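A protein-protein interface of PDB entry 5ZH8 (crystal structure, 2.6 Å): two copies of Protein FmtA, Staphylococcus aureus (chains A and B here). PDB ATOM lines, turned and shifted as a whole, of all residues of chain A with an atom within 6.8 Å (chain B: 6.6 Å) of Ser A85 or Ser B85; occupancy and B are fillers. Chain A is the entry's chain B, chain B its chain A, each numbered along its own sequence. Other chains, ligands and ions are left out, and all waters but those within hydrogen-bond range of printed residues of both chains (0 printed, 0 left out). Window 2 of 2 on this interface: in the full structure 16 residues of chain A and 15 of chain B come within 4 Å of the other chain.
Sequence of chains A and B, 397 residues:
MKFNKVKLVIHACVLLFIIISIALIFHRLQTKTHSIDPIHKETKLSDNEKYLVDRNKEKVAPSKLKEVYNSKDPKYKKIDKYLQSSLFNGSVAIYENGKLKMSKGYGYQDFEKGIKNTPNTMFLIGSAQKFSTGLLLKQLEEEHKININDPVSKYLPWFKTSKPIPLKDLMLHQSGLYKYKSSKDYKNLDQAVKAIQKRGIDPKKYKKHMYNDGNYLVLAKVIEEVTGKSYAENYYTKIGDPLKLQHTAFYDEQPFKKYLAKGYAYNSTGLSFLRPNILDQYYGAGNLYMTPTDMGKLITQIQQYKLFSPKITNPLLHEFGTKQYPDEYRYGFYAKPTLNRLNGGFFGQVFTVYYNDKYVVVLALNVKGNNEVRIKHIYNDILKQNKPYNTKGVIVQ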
ATOM      1  N   ASP A  80      22.242  22.888 -16.477  1.00  0.00           N
ATOM      2  CA  ASP A  80      21.607  22.810 -17.783  1.00  0.00           C
ATOM      3  C   ASP A  80      21.959  24.038 -18.614  1.00  0.00           C
ATOM      4  O   ASP A  80      22.308  23.933 -19.782  1.00  0.00           O
ATOM      5  CB  ASP A  80      20.090  22.718 -17.626  1.00  0.00           C
ATOM      6  CG  ASP A  80      19.368  22.726 -18.959  1.00  0.00           C
ATOM      7  OD1 ASP A  80      19.394  21.707 -19.673  1.00  0.00           O
ATOM      8  OD2 ASP A  80      18.759  23.759 -19.284  1.00  0.00           O
ATOM      9  N   LYS A  81      21.868  25.207 -17.998  1.00  0.00           N
ATOM     10  CA  LYS A  81      22.168  26.459 -18.678  1.00  0.00           C
ATOM     11  C   LYS A  81      23.604  26.468 -19.178  1.00  0.00           C
ATOM     12  O   LYS A  81      23.881  26.921 -20.296  1.00  0.00           O
ATOM     13  CB  LYS A  81      21.924  27.640 -17.740  1.00  0.00           C
ATOM     14  CG  LYS A  81      22.110  28.997 -18.388  1.00  0.00           C
ATOM     15  CD  LYS A  81      21.947  30.104 -17.379  1.00  0.00           C
ATOM     16  CE  LYS A  81      22.131  31.454 -18.047  1.00  0.00           C
ATOM     17  NZ  LYS A  81      22.567  32.491 -17.068  1.00  0.00           N
ATOM     18  N   TYR A  82      24.510  25.966 -18.344  1.00  0.00           N
ATOM     19  CA  TYR A  82      25.903  25.872 -18.726  1.00  0.00           C
ATOM     20  C   TYR A  82      26.071  24.912 -19.904  1.00  0.00           C
ATOM     21  O   TYR A  82      26.718  25.253 -20.897  1.00  0.00           O
ATOM     22  CB  TYR A  82      26.772  25.425 -17.551  1.00  0.00           C
ATOM     23  CG  TYR A  82      28.081  24.858 -18.021  1.00  0.00           C
ATOM     24  CD1 TYR A  82      28.980  25.653 -18.723  1.00  0.00           C
ATOM     25  CD2 TYR A  82      28.404  23.528 -17.802  1.00  0.00           C
ATOM     26  CE1 TYR A  82      30.173  25.142 -19.183  1.00  0.00           C
ATOM     27  CE2 TYR A  82      29.590  23.008 -18.255  1.00  0.00           C
ATOM     28  CZ  TYR A  82      30.478  23.820 -18.945  1.00  0.00           C
ATOM     29  OH  TYR A  82      31.677  23.318 -19.412  1.00  0.00           O
ATOM     30  N   LEU A  83      25.488  23.721 -19.789  1.00  0.00           N
ATOM     31  CA  LEU A  83      25.591  22.709 -20.844  1.00  0.00           C
ATOM     32  C   LEU A  83      25.012  23.184 -22.180  1.00  0.00           C
ATOM     33  O   LEU A  83      25.560  22.895 -23.233  1.00  0.00           O
ATOM     34  CB  LEU A  83      24.912  21.402 -20.421  1.00  0.00           C
ATOM     35  CG  LEU A  83      25.599  20.642 -19.284  1.00  0.00           C
ATOM     36  CD1 LEU A  83      24.829  19.370 -18.963  1.00  0.00           C
ATOM     37  CD2 LEU A  83      27.048  20.314 -19.621  1.00  0.00           C
ATOM     38  N   GLN A  84      23.910  23.920 -22.133  1.00  0.00           N
ATOM     39  CA  GLN A  84      23.313  24.455 -23.353  1.00  0.00           C
ATOM     40  C   GLN A  84      24.169  25.545 -23.971  1.00  0.00           C
ATOM     41  O   GLN A  84      24.500  25.471 -25.147  1.00  0.00           O
ATOM     42  CB  GLN A  84      21.888  24.956 -23.109  1.00  0.00           C
ATOM     43  CG  GLN A  84      20.925  23.826 -22.767  1.00  0.00           C
ATOM     44  CD  GLN A  84      19.500  24.087 -23.185  1.00  0.00           C
ATOM     45  OE1 GLN A  84      19.247  24.392 -24.354  1.00  0.00           O
ATOM     46  NE2 GLN A  84      18.553  23.957 -22.243  1.00  0.00           N
ATOM     47  N   SER A  85      24.549  26.542 -23.185  1.00  0.00           N
ATOM     48  CA  SER A  85      25.306  27.672 -23.731  1.00  0.00           C
ATOM     49  C   SER A  85      26.760  27.319 -24.087  1.00  0.00           C
ATOM     50  O   SER A  85      27.397  28.028 -24.869  1.00  0.00           O
ATOM     51  CB  SER A  85      25.258  28.869 -22.779  1.00  0.00           C
ATOM     52  OG  SER A  85      25.763  28.520 -21.511  1.00  0.00           O
ATOM     53  N   SER A  86      27.281  26.225 -23.533  1.00  0.00           N
ATOM     54  CA  SER A  86      28.609  25.735 -23.918  1.00  0.00           C
ATOM     55  C   SER A  86      28.573  24.755 -25.104  1.00  0.00           C
ATOM     56  O   SER A  86      29.601  24.188 -25.466  1.00  0.00           O
ATOM     57  CB  SER A  86      29.289  25.085 -22.716  1.00  0.00           C
ATOM     58  OG  SER A  86      28.519  24.003 -22.239  1.00  0.00           O
ATOM     59  N   LEU A  87      27.394  24.561 -25.697  1.00  0.00           N
ATOM     60  CA  LEU A  87      27.231  23.742 -26.908  1.00  0.00           C
ATOM     61  C   LEU A  87      27.572  22.269 -26.674  1.00  0.00           C
ATOM     62  O   LEU A  87      28.036  21.580 -27.579  1.00  0.00           O
ATOM     63  CB  LEU A  87      28.067  24.298 -28.075  1.00  0.00           C
ATOM     64  CG  LEU A  87      27.660  25.626 -28.716  1.00  0.00           C
ATOM     65  CD1 LEU A  87      27.030  26.606 -27.751  1.00  0.00           C
ATOM     66  CD2 LEU A  87      28.864  26.264 -29.391  1.00  0.00           C
ATOM     67  N   PHE A  88      27.338  21.803 -25.452  1.00  0.00           N
ATOM     68  CA  PHE A  88      27.591  20.417 -25.066  1.00  0.00           C
ATOM     69  C   PHE A  88      26.813  19.472 -25.982  1.00  0.00           C
ATOM     70  O   PHE A  88      25.622  19.658 -26.196  1.00  0.00           O
ATOM     71  CB  PHE A  88      27.156  20.223 -23.611  1.00  0.00           C
ATOM     72  CG  PHE A  88      27.319  18.827 -23.091  1.00  0.00           C
ATOM     73  CD1 PHE A  88      28.577  18.269 -22.952  1.00  0.00           C
ATOM     74  CD2 PHE A  88      26.210  18.085 -22.688  1.00  0.00           C
ATOM     75  CE1 PHE A  88      28.735  16.984 -22.448  1.00  0.00           C
ATOM     76  CE2 PHE A  88      26.357  16.799 -22.184  1.00  0.00           C
ATOM     77  CZ  PHE A  88      27.624  16.250 -22.064  1.00  0.00           C
ATOM     78  N   ARG A 374      34.402  20.624 -18.148  1.00  0.00           N
ATOM     79  CA  ARG A 374      32.956  20.675 -17.960  1.00  0.00           C
ATOM     80  C   ARG A 374      32.548  20.035 -16.641  1.00  0.00           C
ATOM     81  O   ARG A 374      31.845  20.640 -15.848  1.00  0.00           O
ATOM     82  CB  ARG A 374      32.213  19.969 -19.104  1.00  0.00           C
ATOM     83  CG  ARG A 374      32.442  20.535 -20.495  1.00  0.00           C
ATOM     84  CD  ARG A 374      31.756  19.655 -21.529  1.00  0.00           C
ATOM     85  NE  ARG A 374      31.748  20.229 -22.871  1.00  0.00           N
ATOM     86  CZ  ARG A 374      30.965  21.230 -23.260  1.00  0.00           C
ATOM     87  NH1 ARG A 374      30.123  21.803 -22.411  1.00  0.00           N
ATOM     88  NH2 ARG A 374      31.023  21.667 -24.506  1.00  0.00           N
ATOM     89  N   HIS A 377      33.605  21.991 -13.627  1.00  0.00           N
ATOM     90  CA  HIS A 377      32.798  23.176 -13.433  1.00  0.00           C
ATOM     91  C   HIS A 377      31.490  22.807 -12.753  1.00  0.00           C
ATOM     92  O   HIS A 377      30.997  23.552 -11.915  1.00  0.00           O
ATOM     93  CB  HIS A 377      32.543  23.855 -14.771  1.00  0.00           C
ATOM     94  CG  HIS A 377      31.721  25.095 -14.661  1.00  0.00           C
ATOM     95  ND1 HIS A 377      32.183  26.238 -14.051  1.00  0.00           N
ATOM     96  CD2 HIS A 377      30.457  25.365 -15.072  1.00  0.00           C
ATOM     97  CE1 HIS A 377      31.244  27.167 -14.105  1.00  0.00           C
ATOM     98  NE2 HIS A 377      30.184  26.660 -14.712  1.00  0.00           N
ATOM     99  N   ASP B  80      31.341  37.426 -26.552  1.00  0.00           N
ATOM    100  CA  ASP B  80      32.003  37.513 -25.269  1.00  0.00           C
ATOM    101  C   ASP B  80      31.278  36.669 -24.229  1.00  0.00           C
ATOM    102  O   ASP B  80      31.893  35.892 -23.488  1.00  0.00           O
ATOM    103  CB  ASP B  80      32.058  38.974 -24.811  1.00  0.00           C
ATOM    104  CG  ASP B  80      32.672  39.132 -23.442  1.00  0.00           C
ATOM    105  OD1 ASP B  80      33.906  38.947 -23.297  1.00  0.00           O
ATOM    106  OD2 ASP B  80      31.908  39.424 -22.509  1.00  0.00           O
ATOM    107  N   LYS B  81      29.962  36.825 -24.191  1.00  0.00           N
ATOM    108  CA  LYS B  81      29.139  36.102 -23.236  1.00  0.00           C
ATOM    109  C   LYS B  81      29.263  34.602 -23.442  1.00  0.00           C
ATOM    110  O   LYS B  81      29.326  33.834 -22.487  1.00  0.00           O
ATOM    111  CB  LYS B  81      27.683  36.534 -23.375  1.00  0.00           C
ATOM    112  CG  LYS B  81      26.779  35.990 -22.296  1.00  0.00           C
ATOM    113  CD  LYS B  81      25.447  36.716 -22.308  1.00  0.00           C
ATOM    114  CE  LYS B  81      24.674  36.476 -21.020  1.00  0.00           C
ATOM    115  NZ  LYS B  81      25.304  37.104 -19.815  1.00  0.00           N
ATOM    116  N   TYR B  82      29.290  34.190 -24.699  1.00  0.00           N
ATOM    117  CA  TYR B  82      29.453  32.784 -25.036  1.00  0.00           C
ATOM    118  C   TYR B  82      30.815  32.287 -24.580  1.00  0.00           C
ATOM    119  O   TYR B  82      30.903  31.252 -23.926  1.00  0.00           O
ATOM    120  CB  TYR B  82      29.275  32.542 -26.535  1.00  0.00           C
ATOM    121  CG  TYR B  82      29.903  31.260 -26.973  1.00  0.00           C
ATOM    122  CD1 TYR B  82      29.449  30.052 -26.481  1.00  0.00           C
ATOM    123  CD2 TYR B  82      30.976  31.255 -27.854  1.00  0.00           C
ATOM    124  CE1 TYR B  82      30.034  28.864 -26.851  1.00  0.00           C
ATOM    125  CE2 TYR B  82      31.572  30.066 -28.248  1.00  0.00           C
ATOM    126  CZ  TYR B  82      31.104  28.877 -27.735  1.00  0.00           C
ATOM    127  OH  TYR B  82      31.694  27.703 -28.126  1.00  0.00           O
ATOM    128  N   LEU B  83      31.870  33.024 -24.914  1.00  0.00           N
ATOM    129  CA  LEU B  83      33.234  32.626 -24.545  1.00  0.00           C
ATOM    130  C   LEU B  83      33.428  32.545 -23.038  1.00  0.00           C
ATOM    131  O   LEU B  83      34.112  31.643 -22.554  1.00  0.00           O
ATOM    132  CB  LEU B  83      34.268  33.578 -25.145  1.00  0.00           C
ATOM    133  CG  LEU B  83      34.402  33.532 -26.667  1.00  0.00           C
ATOM    134  CD1 LEU B  83      35.453  34.535 -27.110  1.00  0.00           C
ATOM    135  CD2 LEU B  83      34.747  32.133 -27.152  1.00  0.00           C
ATOM    136  N   GLN B  84      32.826  33.473 -22.295  1.00  0.00           N
ATOM    137  CA  GLN B  84      32.908  33.431 -20.844  1.00  0.00           C
ATOM    138  C   GLN B  84      32.146  32.237 -20.265  1.00  0.00           C
ATOM    139  O   GLN B  84      32.705  31.461 -19.496  1.00  0.00           O
ATOM    140  CB  GLN B  84      32.390  34.722 -20.230  1.00  0.00           C
ATOM    141  CG  GLN B  84      33.278  35.926 -20.452  1.00  0.00           C
ATOM    142  CD  GLN B  84      32.938  37.075 -19.500  1.00  0.00           C
ATOM    143  OE1 GLN B  84      32.517  36.871 -18.347  1.00  0.00           O
ATOM    144  NE2 GLN B  84      33.119  38.302 -19.987  1.00  0.00           N
ATOM    145  N   SER B  85      30.883  32.075 -20.641  1.00  0.00           N
ATOM    146  CA  SER B  85      30.061  31.015 -20.054  1.00  0.00           C
ATOM    147  C   SER B  85      30.436  29.609 -20.543  1.00  0.00           C
ATOM    148  O   SER B  85      30.108  28.619 -19.894  1.00  0.00           O
ATOM    149  CB  SER B  85      28.574  31.288 -20.288  1.00  0.00           C
ATOM    150  OG  SER B  85      28.296  31.404 -21.661  1.00  0.00           O
ATOM    151  N   SER B  86      31.138  29.517 -21.668  1.00  0.00           N
ATOM    152  CA  SER B  86      31.656  28.228 -22.141  1.00  0.00           C
ATOM    153  C   SER B  86      33.052  27.898 -21.585  1.00  0.00           C
ATOM    154  O   SER B  86      33.648  26.897 -21.966  1.00  0.00           O
ATOM    155  CB  SER B  86      31.678  28.199 -23.669  1.00  0.00           C
ATOM    156  OG  SER B  86      32.494  29.235 -24.171  1.00  0.00           O
ATOM    157  N   LEU B  87      33.560  28.738 -20.686  1.00  0.00           N
ATOM    158  CA  LEU B  87      34.831  28.498 -19.990  1.00  0.00           C
ATOM    159  C   LEU B  87      36.027  28.476 -20.934  1.00  0.00           C
ATOM    160  O   LEU B  87      37.001  27.786 -20.692  1.00  0.00           O
ATOM    161  CB  LEU B  87      34.768  27.203 -19.171  1.00  0.00           C
ATOM    162  CG  LEU B  87      33.552  27.045 -18.252  1.00  0.00           C
ATOM    163  CD1 LEU B  87      33.495  25.642 -17.667  1.00  0.00           C
ATOM    164  CD2 LEU B  87      33.582  28.102 -17.163  1.00  0.00           C
ATOM    165  N   PHE B  88      35.935  29.251 -22.009  1.00  0.00           N
ATOM    166  CA  PHE B  88      36.995  29.372 -23.007  1.00  0.00           C
ATOM    167  C   PHE B  88      38.286  29.816 -22.336  1.00  0.00           C
ATOM    168  O   PHE B  88      38.283  30.778 -21.569  1.00  0.00           O
ATOM    169  CB  PHE B  88      36.565  30.398 -24.057  1.00  0.00           C
ATOM    170  CG  PHE B  88      37.584  30.655 -25.130  1.00  0.00           C
ATOM    171  CD1 PHE B  88      37.961  29.652 -26.017  1.00  0.00           C
ATOM    172  CD2 PHE B  88      38.136  31.925 -25.284  1.00  0.00           C
ATOM    173  CE1 PHE B  88      38.887  29.909 -27.022  1.00  0.00           C
ATOM    174  CE2 PHE B  88      39.057  32.184 -26.288  1.00  0.00           C
ATOM    175  CZ  PHE B  88      39.435  31.175 -27.156  1.00  0.00           C
ATOM    176  N   HIS B 377      30.262  28.484 -34.124  1.00  0.00           N
ATOM    177  CA  HIS B 377      29.156  29.125 -33.447  1.00  0.00           C
ATOM    178  C   HIS B 377      29.266  30.635 -33.594  1.00  0.00           C
ATOM    179  O   HIS B 377      28.266  31.322 -33.759  1.00  0.00           O
ATOM    180  CB  HIS B 377      29.134  28.727 -31.979  1.00  0.00           C
ATOM    181  CG  HIS B 377      28.021  29.351 -31.205  1.00  0.00           C
ATOM    182  ND1 HIS B 377      26.696  29.045 -31.429  1.00  0.00           N
ATOM    183  CD2 HIS B 377      28.034  30.262 -30.205  1.00  0.00           C
ATOM    184  CE1 HIS B 377      25.940  29.745 -30.605  1.00  0.00           C
ATOM    185  NE2 HIS B 377      26.727  30.483 -29.845  1.00  0.00           N
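Of the printed residues of chain B, Tyr A82 touches Ser B85 and Leu B87. Ser A85 touches just these residues of chain B: Tyr B82 (3.3 Å) and Ser B85 (3.8 Å). Of the printed residues of chain B, Leu A87 touches Tyr B82 and His B377. Lys B81 touches none of the printed residues of chain A. Printed residues of chain A within 4 Å of Tyr B82: Ser A85 and Leu A87. Printed residues of chain A within 4 Å of Ser B86: Ser A86 (3.9 Å). The nearest residue of chain B that does not touch Ser A85 is Ser B86 (4.4 Å). The nearest residue of chain A that does not touch Ser B85 is Ser A86 (4.6 Å).
Of the 10 printed residues of chain B, 5 touch a printed residue of chain A. Hydrophobic or aromatic side chains of chain B within 4 Å of the printed part of chain A: Tyr B82, Leu B87 and His B377. Of the 11 printed residues of chain A, 5 touch a printed residue of chain B. Printed residues of chain A that touch a printed residue of chain B: Tyr A82, Ser A85, Ser A86, Leu A87 and His A377. Hydrophobic or aromatic side chains of chain A within 4 Å of the printed part of chain B: Tyr A82, Leu A87 and His A377.
Tyr A82 touches Ser B85, and with the chains exchanged Ser A85 touches Tyr B82. Tyr A82 touches Leu B87, and with the chains exchanged Leu A87 touches Tyr B82. Ser A85 touches its own counterpart, Ser B85. Leu A87 touches His B377, and with the chains exchanged His A377 touches Leu B87. 10 positions are printed for both chains.
O of Leu B83 sits at hydrogen-bond distance from OG of Ser B86, 3.3 Å away. The backbone carbonyl oxygen (O) of Tyr A82 lies within hydrogen-bond range of the side-chain hydroxyl (OG) of Ser A86. The guanidinium group (NH1) of Arg A374 is in hydrogen-bond range of the side-chain hydroxyl (OG) of Ser A86 (2.7 Å). O of Tyr B82 sits at hydrogen-bond distance from OG of Ser B86. O of Tyr B82 sits at hydrogen-bond distance from OG of Ser B85 (3.5 Å). The backbone carbonyl oxygen (O) of Leu A83 lies within hydrogen-bond range of the side-chain hydroxyl (OG) of Ser A86.
Among the printed residues, merely in contact across the chains: Tyr A82 with Ser B85 (3.4 Å), Tyr A82 with Leu B87 (3.4 Å), Ser A85 with Tyr B82 (3.3 Å), Ser A85 with Ser B85 (3.8 Å), Ser A86 with Ser B86 (3.9 Å), Leu A87 with Tyr B82 (3.4 Å), Leu A87 with His B377 (3.6 Å) and His A377 with Leu B87 (3.5 Å).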
